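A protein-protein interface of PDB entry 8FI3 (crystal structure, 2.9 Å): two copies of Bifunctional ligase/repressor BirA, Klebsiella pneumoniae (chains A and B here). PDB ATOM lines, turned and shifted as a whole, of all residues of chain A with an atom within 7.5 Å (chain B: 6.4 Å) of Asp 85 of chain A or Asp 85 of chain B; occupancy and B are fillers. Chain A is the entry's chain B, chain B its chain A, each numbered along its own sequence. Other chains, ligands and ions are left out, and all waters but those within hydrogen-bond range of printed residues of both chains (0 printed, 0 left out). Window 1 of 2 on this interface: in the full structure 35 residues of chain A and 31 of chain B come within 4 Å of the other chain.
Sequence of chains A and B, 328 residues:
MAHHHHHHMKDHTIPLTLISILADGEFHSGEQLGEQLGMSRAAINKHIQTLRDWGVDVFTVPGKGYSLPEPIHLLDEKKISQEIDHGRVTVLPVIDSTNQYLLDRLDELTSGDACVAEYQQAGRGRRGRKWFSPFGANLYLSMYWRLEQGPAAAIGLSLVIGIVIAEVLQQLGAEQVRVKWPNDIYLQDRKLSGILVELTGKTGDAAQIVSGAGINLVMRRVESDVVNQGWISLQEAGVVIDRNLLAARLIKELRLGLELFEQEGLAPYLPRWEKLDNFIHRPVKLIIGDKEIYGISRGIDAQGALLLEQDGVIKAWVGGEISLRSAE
NZ of Lys 252 of chain A lies within salt-bridge range of OE1 of Glu 83 of chain B. OD1 of Asp 85 of chain A lies close to OD1 of Asp 85 of chain B (2.6 Å).
O of Glu 83 of chain B lies close to ND1 of His 86 of chain B, at 3.3 Å. The guanidinium group (NH1) of Arg 255 of chain B lies within salt-bridge range of the side-chain carboxylate (OD1) of Asp 85 of chain B (3.9 Å). The backbone carbonyl oxygen (O) of His 86 of chain A is in hydrogen-bond range of the guanidinium group (NE) of Arg 255 of chain A (3.4 Å). NH2 of Arg 255 of chain A lies close to O of Gly 87 of chain A, at 3.2 Å. The backbone carbonyl oxygen of Arg 88 of chain A is in hydrogen-bond range of the guanidinium group of Arg 255 of chain A (3.0 Å). O of Gly 112 of chain A is in hydrogen-bond range of NE of Arg 255 of chain A, 2.8 Å away.
Asp 85 of chain B touches Ile 84 of chain A (OD1 to CG2, 3.1 Å). CG2 of Ile 84 of chain B touches OD1 of Asp 85 of chain A, 3.9 Å away. Ile 84 of chain B touches Val 89 of chain A (CD1 to CG2, 3.99 Å). Ala 248 of chain A touches Ile 80 of chain B. Ala 248 of chain A touches Glu 83 of chain B (CB to CB, 3.5 Å). Ala 248 of chain A touches Ile 84 of chain B. Ile 84 of chain B touches Ile 251 of chain A. Arg 255 of chain A touches Ile 84 of chain B (NH1 to CG2, 3.6 Å).
Asp 85 of chain A touches just these residues of chain B: Ile 84 (3.9 Å) and Asp 85 (2.6 Å). Of chain A, only Ile 84 and Asp 85 come within 4 Å of Asp 85 of chain B. Of the printed residues of chain A, Glu 83 of chain B touches Ala 248 (3.5 Å) and Lys 252 (3.1 Å). Of the printed residues of chain B, Ala 248 of chain A touches Ile 80 (3.2 Å), Glu 83 (3.5 Å) and Ile 84 (3.7 Å). Of the printed residues of chain B, Arg 255 of chain A touches Ile 84 (3.6 Å). Of the printed residues of chain A, Ile 80 of chain B touches Ala 248. Asp 113 of chain A touches none of the printed residues of chain B. The nearest residue of chain A that does not touch Asp 85 of chain B is Ser 81 of chain A (5.4 Å).
Printed residues of chain B that touch a printed residue of chain A: Ile 80, Glu 83, Ile 84 and Asp 85. Hydrophobic or aromatic side chains of chain B that line the printed part of chain A: Ile 80 and Ile 84. Of the 21 printed residues of chain A, 7 touch a printed residue of chain B. Hydrophobic or aromatic side chains of chain A within 4 Å of the printed part of chain B: Ile 84, Val 89, Ala 248 and Ile 251. Among the printed residues, 10 pairs touch across the chains.
Ile 84 of chain A touches Asp 85 of chain B, and with the chains exchanged Asp 85 of chain A touches Ile 84 of chain B. Asp 85 of chain B touches its own counterpart, Asp 85 of chain A. Arg 255 of chain A touches Ile 84 of chain B, but with the chains exchanged Ile 84 of chain A does not touch Arg 255 of chain B (4.04 Å). Positions printed for both chains: 80, 81, 82, 83, 84, 85, 86, 87, 88, 111, 112 and 255. Of the 10 pairs that touch across the chains among the printed residues, 3 have their exchanged pair printed and touching as well.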
ATOM      1  N   LYS A  79      13.332  31.989   6.115  1.00  0.00           N
ATOM      2  CA  LYS A  79      12.353  32.378   7.127  1.00  0.00           C
ATOM      3  C   LYS A  79      11.595  31.168   7.661  1.00  0.00           C
ATOM      4  O   LYS A  79      11.378  31.049   8.872  1.00  0.00           O
ATOM      5  CB  LYS A  79      11.380  33.405   6.547  1.00  0.00           C
ATOM      6  CG  LYS A  79      11.693  34.846   6.923  1.00  0.00           C
ATOM      7  CD  LYS A  79      10.649  35.802   6.361  1.00  0.00           C
ATOM      8  CE  LYS A  79      11.123  36.442   5.065  1.00  0.00           C
ATOM      9  NZ  LYS A  79       9.983  36.826   4.184  1.00  0.00           N
ATOM     10  N   ILE A  80      11.185  30.263   6.771  1.00  0.00           N
ATOM     11  CA  ILE A  80      10.444  29.078   7.194  1.00  0.00           C
ATOM     12  C   ILE A  80      11.321  28.164   8.041  1.00  0.00           C
ATOM     13  O   ILE A  80      10.884  27.651   9.078  1.00  0.00           O
ATOM     14  CB  ILE A  80       9.873  28.343   5.967  1.00  0.00           C
ATOM     15  CG1 ILE A  80       8.664  29.095   5.411  1.00  0.00           C
ATOM     16  CG2 ILE A  80       9.490  26.915   6.321  1.00  0.00           C
ATOM     17  CD1 ILE A  80       8.254  28.654   4.024  1.00  0.00           C
ATOM     18  N   SER A  81      12.569  27.947   7.618  1.00  0.00           N
ATOM     19  CA  SER A  81      13.452  27.046   8.353  1.00  0.00           C
ATOM     20  C   SER A  81      13.736  27.558   9.759  1.00  0.00           C
ATOM     21  O   SER A  81      13.772  26.775  10.714  1.00  0.00           O
ATOM     22  CB  SER A  81      14.757  26.848   7.583  1.00  0.00           C
ATOM     23  OG  SER A  81      14.506  26.444   6.249  1.00  0.00           O
ATOM     24  N   GLN A  82      13.939  28.871   9.908  1.00  0.00           N
ATOM     25  CA  GLN A  82      14.245  29.419  11.226  1.00  0.00           C
ATOM     26  C   GLN A  82      13.087  29.213  12.192  1.00  0.00           C
ATOM     27  O   GLN A  82      13.296  28.846  13.352  1.00  0.00           O
ATOM     28  CB  GLN A  82      14.603  30.901  11.126  1.00  0.00           C
ATOM     29  CG  GLN A  82      15.366  31.407  12.342  1.00  0.00           C
ATOM     30  CD  GLN A  82      14.835  32.725  12.857  1.00  0.00           C
ATOM     31  OE1 GLN A  82      14.943  33.754  12.192  1.00  0.00           O
ATOM     32  NE2 GLN A  82      14.253  32.701  14.053  1.00  0.00           N
ATOM     33  N   GLU A  83      11.854  29.449  11.734  1.00  0.00           N
ATOM     34  CA  GLU A  83      10.706  29.199  12.598  1.00  0.00           C
ATOM     35  C   GLU A  83      10.578  27.716  12.912  1.00  0.00           C
ATOM     36  O   GLU A  83      10.114  27.349  13.998  1.00  0.00           O
ATOM     37  CB  GLU A  83       9.429  29.724  11.942  1.00  0.00           C
ATOM     38  CG  GLU A  83       8.227  29.786  12.871  1.00  0.00           C
ATOM     39  CD  GLU A  83       8.377  30.840  13.955  1.00  0.00           C
ATOM     40  OE1 GLU A  83       9.107  31.829  13.730  1.00  0.00           O
ATOM     41  OE2 GLU A  83       7.764  30.679  15.029  1.00  0.00           O
ATOM     42  N   ILE A  84      10.970  26.855  11.974  1.00  0.00           N
ATOM     43  CA  ILE A  84      11.007  25.422  12.236  1.00  0.00           C
ATOM     44  C   ILE A  84      12.115  25.088  13.233  1.00  0.00           C
ATOM     45  O   ILE A  84      11.957  24.208  14.088  1.00  0.00           O
ATOM     46  CB  ILE A  84      11.176  24.654  10.908  1.00  0.00           C
ATOM     47  CG1 ILE A  84       9.829  24.479  10.209  1.00  0.00           C
ATOM     48  CG2 ILE A  84      11.805  23.300  11.137  1.00  0.00           C
ATOM     49  CD1 ILE A  84       9.943  24.138   8.739  1.00  0.00           C
ATOM     50  N   ASP A  85      13.237  25.806  13.158  1.00  0.00           N
ATOM     51  CA  ASP A  85      14.464  25.468  13.874  1.00  0.00           C
ATOM     52  C   ASP A  85      14.775  26.333  15.085  1.00  0.00           C
ATOM     53  O   ASP A  85      15.421  25.842  16.013  1.00  0.00           O
ATOM     54  CB  ASP A  85      15.660  25.540  12.921  1.00  0.00           C
ATOM     55  CG  ASP A  85      15.923  24.232  12.229  1.00  0.00           C
ATOM     56  OD1 ASP A  85      15.349  23.222  12.673  1.00  0.00           O
ATOM     57  OD2 ASP A  85      16.712  24.211  11.260  1.00  0.00           O
ATOM     58  N   HIS A  86      14.305  27.579  15.117  1.00  0.00           N
ATOM     59  CA  HIS A  86      14.771  28.581  16.076  1.00  0.00           C
ATOM     60  C   HIS A  86      16.298  28.587  16.156  1.00  0.00           C
ATOM     61  O   HIS A  86      16.894  28.399  17.221  1.00  0.00           O
ATOM     62  CB  HIS A  86      14.173  28.331  17.462  1.00  0.00           C
ATOM     63  CG  HIS A  86      12.680  28.409  17.512  1.00  0.00           C
ATOM     64  ND1 HIS A  86      11.975  29.549  17.194  1.00  0.00           N
ATOM     65  CD2 HIS A  86      11.756  27.471  17.829  1.00  0.00           C
ATOM     66  CE1 HIS A  86      10.680  29.313  17.326  1.00  0.00           C
ATOM     67  NE2 HIS A  86      10.521  28.059  17.707  1.00  0.00           N
ATOM     68  N   GLY A  87      16.931  28.811  15.014  1.00  0.00           N
ATOM     69  CA  GLY A  87      18.379  28.915  14.943  1.00  0.00           C
ATOM     70  C   GLY A  87      18.985  28.210  13.745  1.00  0.00           C
ATOM     71  O   GLY A  87      18.450  27.229  13.225  1.00  0.00           O
ATOM     72  N   ARG A  88      20.131  28.712  13.296  1.00  0.00           N
ATOM     73  CA  ARG A  88      20.905  28.084  12.236  1.00  0.00           C
ATOM     74  C   ARG A  88      22.121  27.372  12.824  1.00  0.00           C
ATOM     75  O   ARG A  88      22.468  27.538  13.995  1.00  0.00           O
ATOM     76  CB  ARG A  88      21.346  29.121  11.196  1.00  0.00           C
ATOM     77  CG  ARG A  88      20.203  29.820  10.478  1.00  0.00           C
ATOM     78  CD  ARG A  88      20.159  31.303  10.817  1.00  0.00           C
ATOM     79  NE  ARG A  88      21.489  31.899  10.855  1.00  0.00           N
ATOM     80  CZ  ARG A  88      21.735  33.168  11.149  1.00  0.00           C
ATOM     81  NH1 ARG A  88      20.756  34.012  11.433  1.00  0.00           N
ATOM     82  NH2 ARG A  88      22.992  33.603  11.161  1.00  0.00           N
ATOM     83  N   VAL A  89      22.774  26.562  11.991  1.00  0.00           N
ATOM     84  CA  VAL A  89      23.958  25.809  12.390  1.00  0.00           C
ATOM     85  C   VAL A  89      25.017  25.952  11.306  1.00  0.00           C
ATOM     86  O   VAL A  89      24.713  25.869  10.111  1.00  0.00           O
ATOM     87  CB  VAL A  89      23.637  24.318  12.641  1.00  0.00           C
ATOM     88  CG1 VAL A  89      24.907  23.543  12.966  1.00  0.00           C
ATOM     89  CG2 VAL A  89      22.627  24.170  13.768  1.00  0.00           C
ATOM     90  N   SER A 111      18.778  34.041  18.676  1.00  0.00           N
ATOM     91  CA  SER A 111      18.788  33.021  19.719  1.00  0.00           C
ATOM     92  C   SER A 111      18.597  31.634  19.123  1.00  0.00           C
ATOM     93  O   SER A 111      17.584  31.358  18.472  1.00  0.00           O
ATOM     94  CB  SER A 111      17.694  33.317  20.746  1.00  0.00           C
ATOM     95  OG  SER A 111      17.653  34.698  21.061  1.00  0.00           O
ATOM     96  N   GLY A 112      19.579  30.762  19.346  1.00  0.00           N
ATOM     97  CA  GLY A 112      19.564  29.410  18.834  1.00  0.00           C
ATOM     98  C   GLY A 112      20.624  29.122  17.791  1.00  0.00           C
ATOM     99  O   GLY A 112      20.873  27.946  17.495  1.00  0.00           O
ATOM    100  N   ASP A 113      21.244  30.153  17.217  1.00  0.00           N
ATOM    101  CA  ASP A 113      22.303  29.936  16.239  1.00  0.00           C
ATOM    102  C   ASP A 113      23.451  29.161  16.874  1.00  0.00           C
ATOM    103  O   ASP A 113      23.926  29.510  17.957  1.00  0.00           O
ATOM    104  CB  ASP A 113      22.798  31.274  15.689  1.00  0.00           C
ATOM    105  CG  ASP A 113      21.882  31.844  14.621  1.00  0.00           C
ATOM    106  OD1 ASP A 113      20.948  31.134  14.192  1.00  0.00           O
ATOM    107  OD2 ASP A 113      22.097  33.005  14.208  1.00  0.00           O
ATOM    108  N   TRP A 145      22.598  33.000  22.486  1.00  0.00           N
ATOM    109  CA  TRP A 145      21.280  33.209  23.073  1.00  0.00           C
ATOM    110  C   TRP A 145      21.213  34.609  23.661  1.00  0.00           C
ATOM    111  O   TRP A 145      22.104  35.011  24.415  1.00  0.00           O
ATOM    112  CB  TRP A 145      20.970  32.168  24.155  1.00  0.00           C
ATOM    113  CG  TRP A 145      19.498  31.962  24.352  1.00  0.00           C
ATOM    114  CD1 TRP A 145      18.691  32.609  25.243  1.00  0.00           C
ATOM    115  CD2 TRP A 145      18.654  31.057  23.631  1.00  0.00           C
ATOM    116  NE1 TRP A 145      17.398  32.158  25.124  1.00  0.00           N
ATOM    117  CE2 TRP A 145      17.349  31.205  24.140  1.00  0.00           C
ATOM    118  CE3 TRP A 145      18.877  30.133  22.604  1.00  0.00           C
ATOM    119  CZ2 TRP A 145      16.272  30.466  23.660  1.00  0.00           C
ATOM    120  CZ3 TRP A 145      17.807  29.399  22.130  1.00  0.00           C
ATOM    121  CH2 TRP A 145      16.520  29.568  22.657  1.00  0.00           C
ATOM    122  N   ALA A 248      23.921  17.214  16.802  1.00  0.00           N
ATOM    123  CA  ALA A 248      22.564  17.584  16.417  1.00  0.00           C
ATOM    124  C   ALA A 248      21.598  17.425  17.583  1.00  0.00           C
ATOM    125  O   ALA A 248      20.731  18.280  17.802  1.00  0.00           O
ATOM    126  CB  ALA A 248      22.111  16.745  15.225  1.00  0.00           C
ATOM    127  N   ILE A 251      22.227  20.343  20.060  1.00  0.00           N
ATOM    128  CA  ILE A 251      21.716  21.618  19.563  1.00  0.00           C
ATOM    129  C   ILE A 251      20.196  21.647  19.640  1.00  0.00           C
ATOM    130  O   ILE A 251      19.597  22.650  20.050  1.00  0.00           O
ATOM    131  CB  ILE A 251      22.216  21.870  18.130  1.00  0.00           C
ATOM    132  CG1 ILE A 251      23.740  21.985  18.105  1.00  0.00           C
ATOM    133  CG2 ILE A 251      21.585  23.122  17.557  1.00  0.00           C
ATOM    134  CD1 ILE A 251      24.312  22.126  16.713  1.00  0.00           C
ATOM    135  N   LYS A 252      19.550  20.546  19.252  1.00  0.00           N
ATOM    136  CA  LYS A 252      18.095  20.471  19.323  1.00  0.00           C
ATOM    137  C   LYS A 252      17.604  20.578  20.763  1.00  0.00           C
ATOM    138  O   LYS A 252      16.703  21.368  21.066  1.00  0.00           O
ATOM    139  CB  LYS A 252      17.616  19.170  18.678  1.00  0.00           C
ATOM    140  CG  LYS A 252      16.209  18.762  19.064  1.00  0.00           C
ATOM    141  CD  LYS A 252      15.839  17.430  18.439  1.00  0.00           C
ATOM    142  CE  LYS A 252      16.582  16.287  19.112  1.00  0.00           C
ATOM    143  NZ  LYS A 252      16.685  15.073  18.248  1.00  0.00           N
ATOM    144  N   ARG A 255      18.253  24.062  22.410  1.00  0.00           N
ATOM    145  CA  ARG A 255      17.313  25.075  21.947  1.00  0.00           C
ATOM    146  C   ARG A 255      15.986  24.968  22.686  1.00  0.00           C
ATOM    147  O   ARG A 255      15.437  25.975  23.145  1.00  0.00           O
ATOM    148  CB  ARG A 255      17.098  24.942  20.439  1.00  0.00           C
ATOM    149  CG  ARG A 255      18.154  25.628  19.593  1.00  0.00           C
ATOM    150  CD  ARG A 255      18.009  25.238  18.134  1.00  0.00           C
ATOM    151  NE  ARG A 255      19.049  25.828  17.300  1.00  0.00           N
ATOM    152  CZ  ARG A 255      19.416  25.354  16.120  1.00  0.00           C
ATOM    153  NH1 ARG A 255      18.851  24.276  15.600  1.00  0.00           N
ATOM    154  NH2 ARG A 255      20.378  25.972  15.442  1.00  0.00           N
ATOM    155  N   LEU A 256      15.467  23.746  22.831  1.00  0.00           N
ATOM    156  CA  LEU A 256      14.205  23.552  23.538  1.00  0.00           C
ATOM    157  C   LEU A 256      14.332  23.929  25.009  1.00  0.00           C
ATOM    158  O   LEU A 256      13.444  24.580  25.572  1.00  0.00           O
ATOM    159  CB  LEU A 256      13.743  22.102  23.402  1.00  0.00           C
ATOM    160  CG  LEU A 256      13.297  21.638  22.017  1.00  0.00           C
ATOM    161  CD1 LEU A 256      12.812  20.201  22.074  1.00  0.00           C
ATOM    162  CD2 LEU A 256      12.214  22.551  21.465  1.00  0.00           C
ATOM    163  N   GLU A 259      14.419  27.899  25.544  1.00  0.00           N
ATOM    164  CA  GLU A 259      13.147  28.607  25.418  1.00  0.00           C
ATOM    165  C   GLU A 259      12.218  28.281  26.579  1.00  0.00           C
ATOM    166  O   GLU A 259      11.454  29.148  27.017  1.00  0.00           O
ATOM    167  CB  GLU A 259      12.460  28.298  24.085  1.00  0.00           C
ATOM    168  CG  GLU A 259      12.593  26.879  23.580  1.00  0.00           C
ATOM    169  CD  GLU A 259      12.429  26.781  22.070  1.00  0.00           C
ATOM    170  OE1 GLU A 259      13.039  27.600  21.349  1.00  0.00           O
ATOM    171  OE2 GLU A 259      11.693  25.886  21.604  1.00  0.00           O
ATOM    172  N   ILE B  80      23.999  16.893  10.299  1.00  0.00           N
ATOM    173  CA  ILE B  80      23.608  17.502  11.564  1.00  0.00           C
ATOM    174  C   ILE B  80      22.232  18.143  11.442  1.00  0.00           C
ATOM    175  O   ILE B  80      21.369  17.963  12.307  1.00  0.00           O
ATOM    176  CB  ILE B  80      24.672  18.516  12.025  1.00  0.00           C
ATOM    177  CG1 ILE B  80      25.947  17.789  12.451  1.00  0.00           C
ATOM    178  CG2 ILE B  80      24.142  19.368  13.167  1.00  0.00           C
ATOM    179  CD1 ILE B  80      27.154  18.691  12.560  1.00  0.00           C
ATOM    180  N   SER B  81      21.997  18.875  10.350  1.00  0.00           N
ATOM    181  CA  SER B  81      20.707  19.531  10.156  1.00  0.00           C
ATOM    182  C   SER B  81      19.581  18.510  10.051  1.00  0.00           C
ATOM    183  O   SER B  81      18.467  18.750  10.530  1.00  0.00           O
ATOM    184  CB  SER B  81      20.742  20.414   8.910  1.00  0.00           C
ATOM    185  OG  SER B  81      21.954  21.144   8.831  1.00  0.00           O
ATOM    186  N   GLN B  82      19.852  17.368   9.414  1.00  0.00           N
ATOM    187  CA  GLN B  82      18.821  16.358   9.224  1.00  0.00           C
ATOM    188  C   GLN B  82      18.307  15.826  10.558  1.00  0.00           C
ATOM    189  O   GLN B  82      17.096  15.689  10.755  1.00  0.00           O
ATOM    190  CB  GLN B  82      19.366  15.213   8.366  1.00  0.00           C
ATOM    191  CG  GLN B  82      18.387  14.069   8.152  1.00  0.00           C
ATOM    192  CD  GLN B  82      17.195  14.472   7.306  1.00  0.00           C
ATOM    193  OE1 GLN B  82      17.311  15.296   6.399  1.00  0.00           O
ATOM    194  NE2 GLN B  82      16.039  13.888   7.599  1.00  0.00           N
ATOM    195  N   GLU B  83      19.210  15.528  11.493  1.00  0.00           N
ATOM    196  CA  GLU B  83      18.766  15.046  12.799  1.00  0.00           C
ATOM    197  C   GLU B  83      18.047  16.128  13.600  1.00  0.00           C
ATOM    198  O   GLU B  83      17.113  15.821  14.348  1.00  0.00           O
ATOM    199  CB  GLU B  83      19.949  14.485  13.587  1.00  0.00           C
ATOM    200  CG  GLU B  83      19.640  13.179  14.315  1.00  0.00           C
ATOM    201  CD  GLU B  83      18.907  13.381  15.631  1.00  0.00           C
ATOM    202  OE1 GLU B  83      18.824  14.534  16.108  1.00  0.00           O
ATOM    203  OE2 GLU B  83      18.398  12.383  16.182  1.00  0.00           O
ATOM    204  N   ILE B  84      18.435  17.395  13.430  1.00  0.00           N
ATOM    205  CA  ILE B  84      17.747  18.479  14.129  1.00  0.00           C
ATOM    206  C   ILE B  84      16.313  18.604  13.634  1.00  0.00           C
ATOM    207  O   ILE B  84      15.401  18.924  14.409  1.00  0.00           O
ATOM    208  CB  ILE B  84      18.532  19.795  13.959  1.00  0.00           C
ATOM    209  CG1 ILE B  84      19.977  19.616  14.440  1.00  0.00           C
ATOM    210  CG2 ILE B  84      17.846  20.932  14.703  1.00  0.00           C
ATOM    211  CD1 ILE B  84      20.652  20.889  14.879  1.00  0.00           C
ATOM    212  N   ASP B  85      16.087  18.334  12.347  1.00  0.00           N
ATOM    213  CA  ASP B  85      14.802  18.551  11.696  1.00  0.00           C
ATOM    214  C   ASP B  85      14.040  17.266  11.406  1.00  0.00           C
ATOM    215  O   ASP B  85      12.801  17.280  11.412  1.00  0.00           O
ATOM    216  CB  ASP B  85      15.008  19.275  10.365  1.00  0.00           C
ATOM    217  CG  ASP B  85      15.186  20.767  10.539  1.00  0.00           C
ATOM    218  OD1 ASP B  85      14.270  21.403  11.088  1.00  0.00           O
ATOM    219  OD2 ASP B  85      16.246  21.282  10.134  1.00  0.00           O
ATOM    220  N   HIS B  86      14.743  16.146  11.193  1.00  0.00           N
ATOM    221  CA  HIS B  86      14.154  14.981  10.523  1.00  0.00           C
ATOM    222  C   HIS B  86      13.331  15.386   9.302  1.00  0.00           C
ATOM    223  O   HIS B  86      12.128  15.121   9.242  1.00  0.00           O
ATOM    224  CB  HIS B  86      13.298  14.090  11.456  1.00  0.00           C
ATOM    225  CG  HIS B  86      13.906  13.830  12.797  1.00  0.00           C
ATOM    226  ND1 HIS B  86      14.011  14.780  13.790  1.00  0.00           N
ATOM    227  CD2 HIS B  86      14.516  12.720  13.274  1.00  0.00           C
ATOM    228  CE1 HIS B  86      14.604  14.247  14.845  1.00  0.00           C
ATOM    229  NE2 HIS B  86      14.928  13.000  14.553  1.00  0.00           N
ATOM    230  N   GLY B  87      13.976  16.016   8.332  1.00  0.00           N
ATOM    231  CA  GLY B  87      13.342  16.388   7.080  1.00  0.00           C
ATOM    232  C   GLY B  87      13.824  17.741   6.599  1.00  0.00           C
ATOM    233  O   GLY B  87      14.170  18.628   7.381  1.00  0.00           O
ATOM    234  N   ARG B  88      13.839  17.908   5.283  1.00  0.00           N
ATOM    235  CA  ARG B  88      14.192  19.165   4.645  1.00  0.00           C
ATOM    236  C   ARG B  88      12.922  19.836   4.139  1.00  0.00           C
ATOM    237  O   ARG B  88      11.848  19.236   4.105  1.00  0.00           O
ATOM    238  CB  ARG B  88      15.184  18.940   3.497  1.00  0.00           C
ATOM    239  N   SER B 111      11.316  10.454   5.593  1.00  0.00           N
ATOM    240  CA  SER B 111      10.117  10.860   6.320  1.00  0.00           C
ATOM    241  C   SER B 111      10.287  12.241   6.936  1.00  0.00           C
ATOM    242  O   SER B 111      11.196  12.469   7.739  1.00  0.00           O
ATOM    243  CB  SER B 111       9.792   9.833   7.408  1.00  0.00           C
ATOM    244  OG  SER B 111       9.620   8.542   6.853  1.00  0.00           O
ATOM    245  N   GLY B 112       9.408  13.164   6.550  1.00  0.00           N
ATOM    246  CA  GLY B 112       9.439  14.529   7.023  1.00  0.00           C
ATOM    247  C   GLY B 112       9.773  15.552   5.960  1.00  0.00           C
ATOM    248  O   GLY B 112       9.568  16.751   6.190  1.00  0.00           O
ATOM    249  N   ARG B 255       5.580  16.672  11.482  1.00  0.00           N
ATOM    250  CA  ARG B 255       6.688  15.761  11.742  1.00  0.00           C
ATOM    251  C   ARG B 255       6.581  15.161  13.139  1.00  0.00           C
ATOM    252  O   ARG B 255       6.755  13.950  13.324  1.00  0.00           O
ATOM    253  CB  ARG B 255       8.021  16.490  11.572  1.00  0.00           C
ATOM    254  CG  ARG B 255       8.448  16.697  10.130  1.00  0.00           C
ATOM    255  CD  ARG B 255       9.629  17.649  10.046  1.00  0.00           C
ATOM    256  NE  ARG B 255      10.024  17.917   8.668  1.00  0.00           N
ATOM    257  CZ  ARG B 255      10.779  18.939   8.291  1.00  0.00           C
ATOM    258  NH1 ARG B 255      11.241  19.815   9.168  1.00  0.00           N
ATOM    259  NH2 ARG B 255      11.071  19.091   7.003  1.00  0.00           N
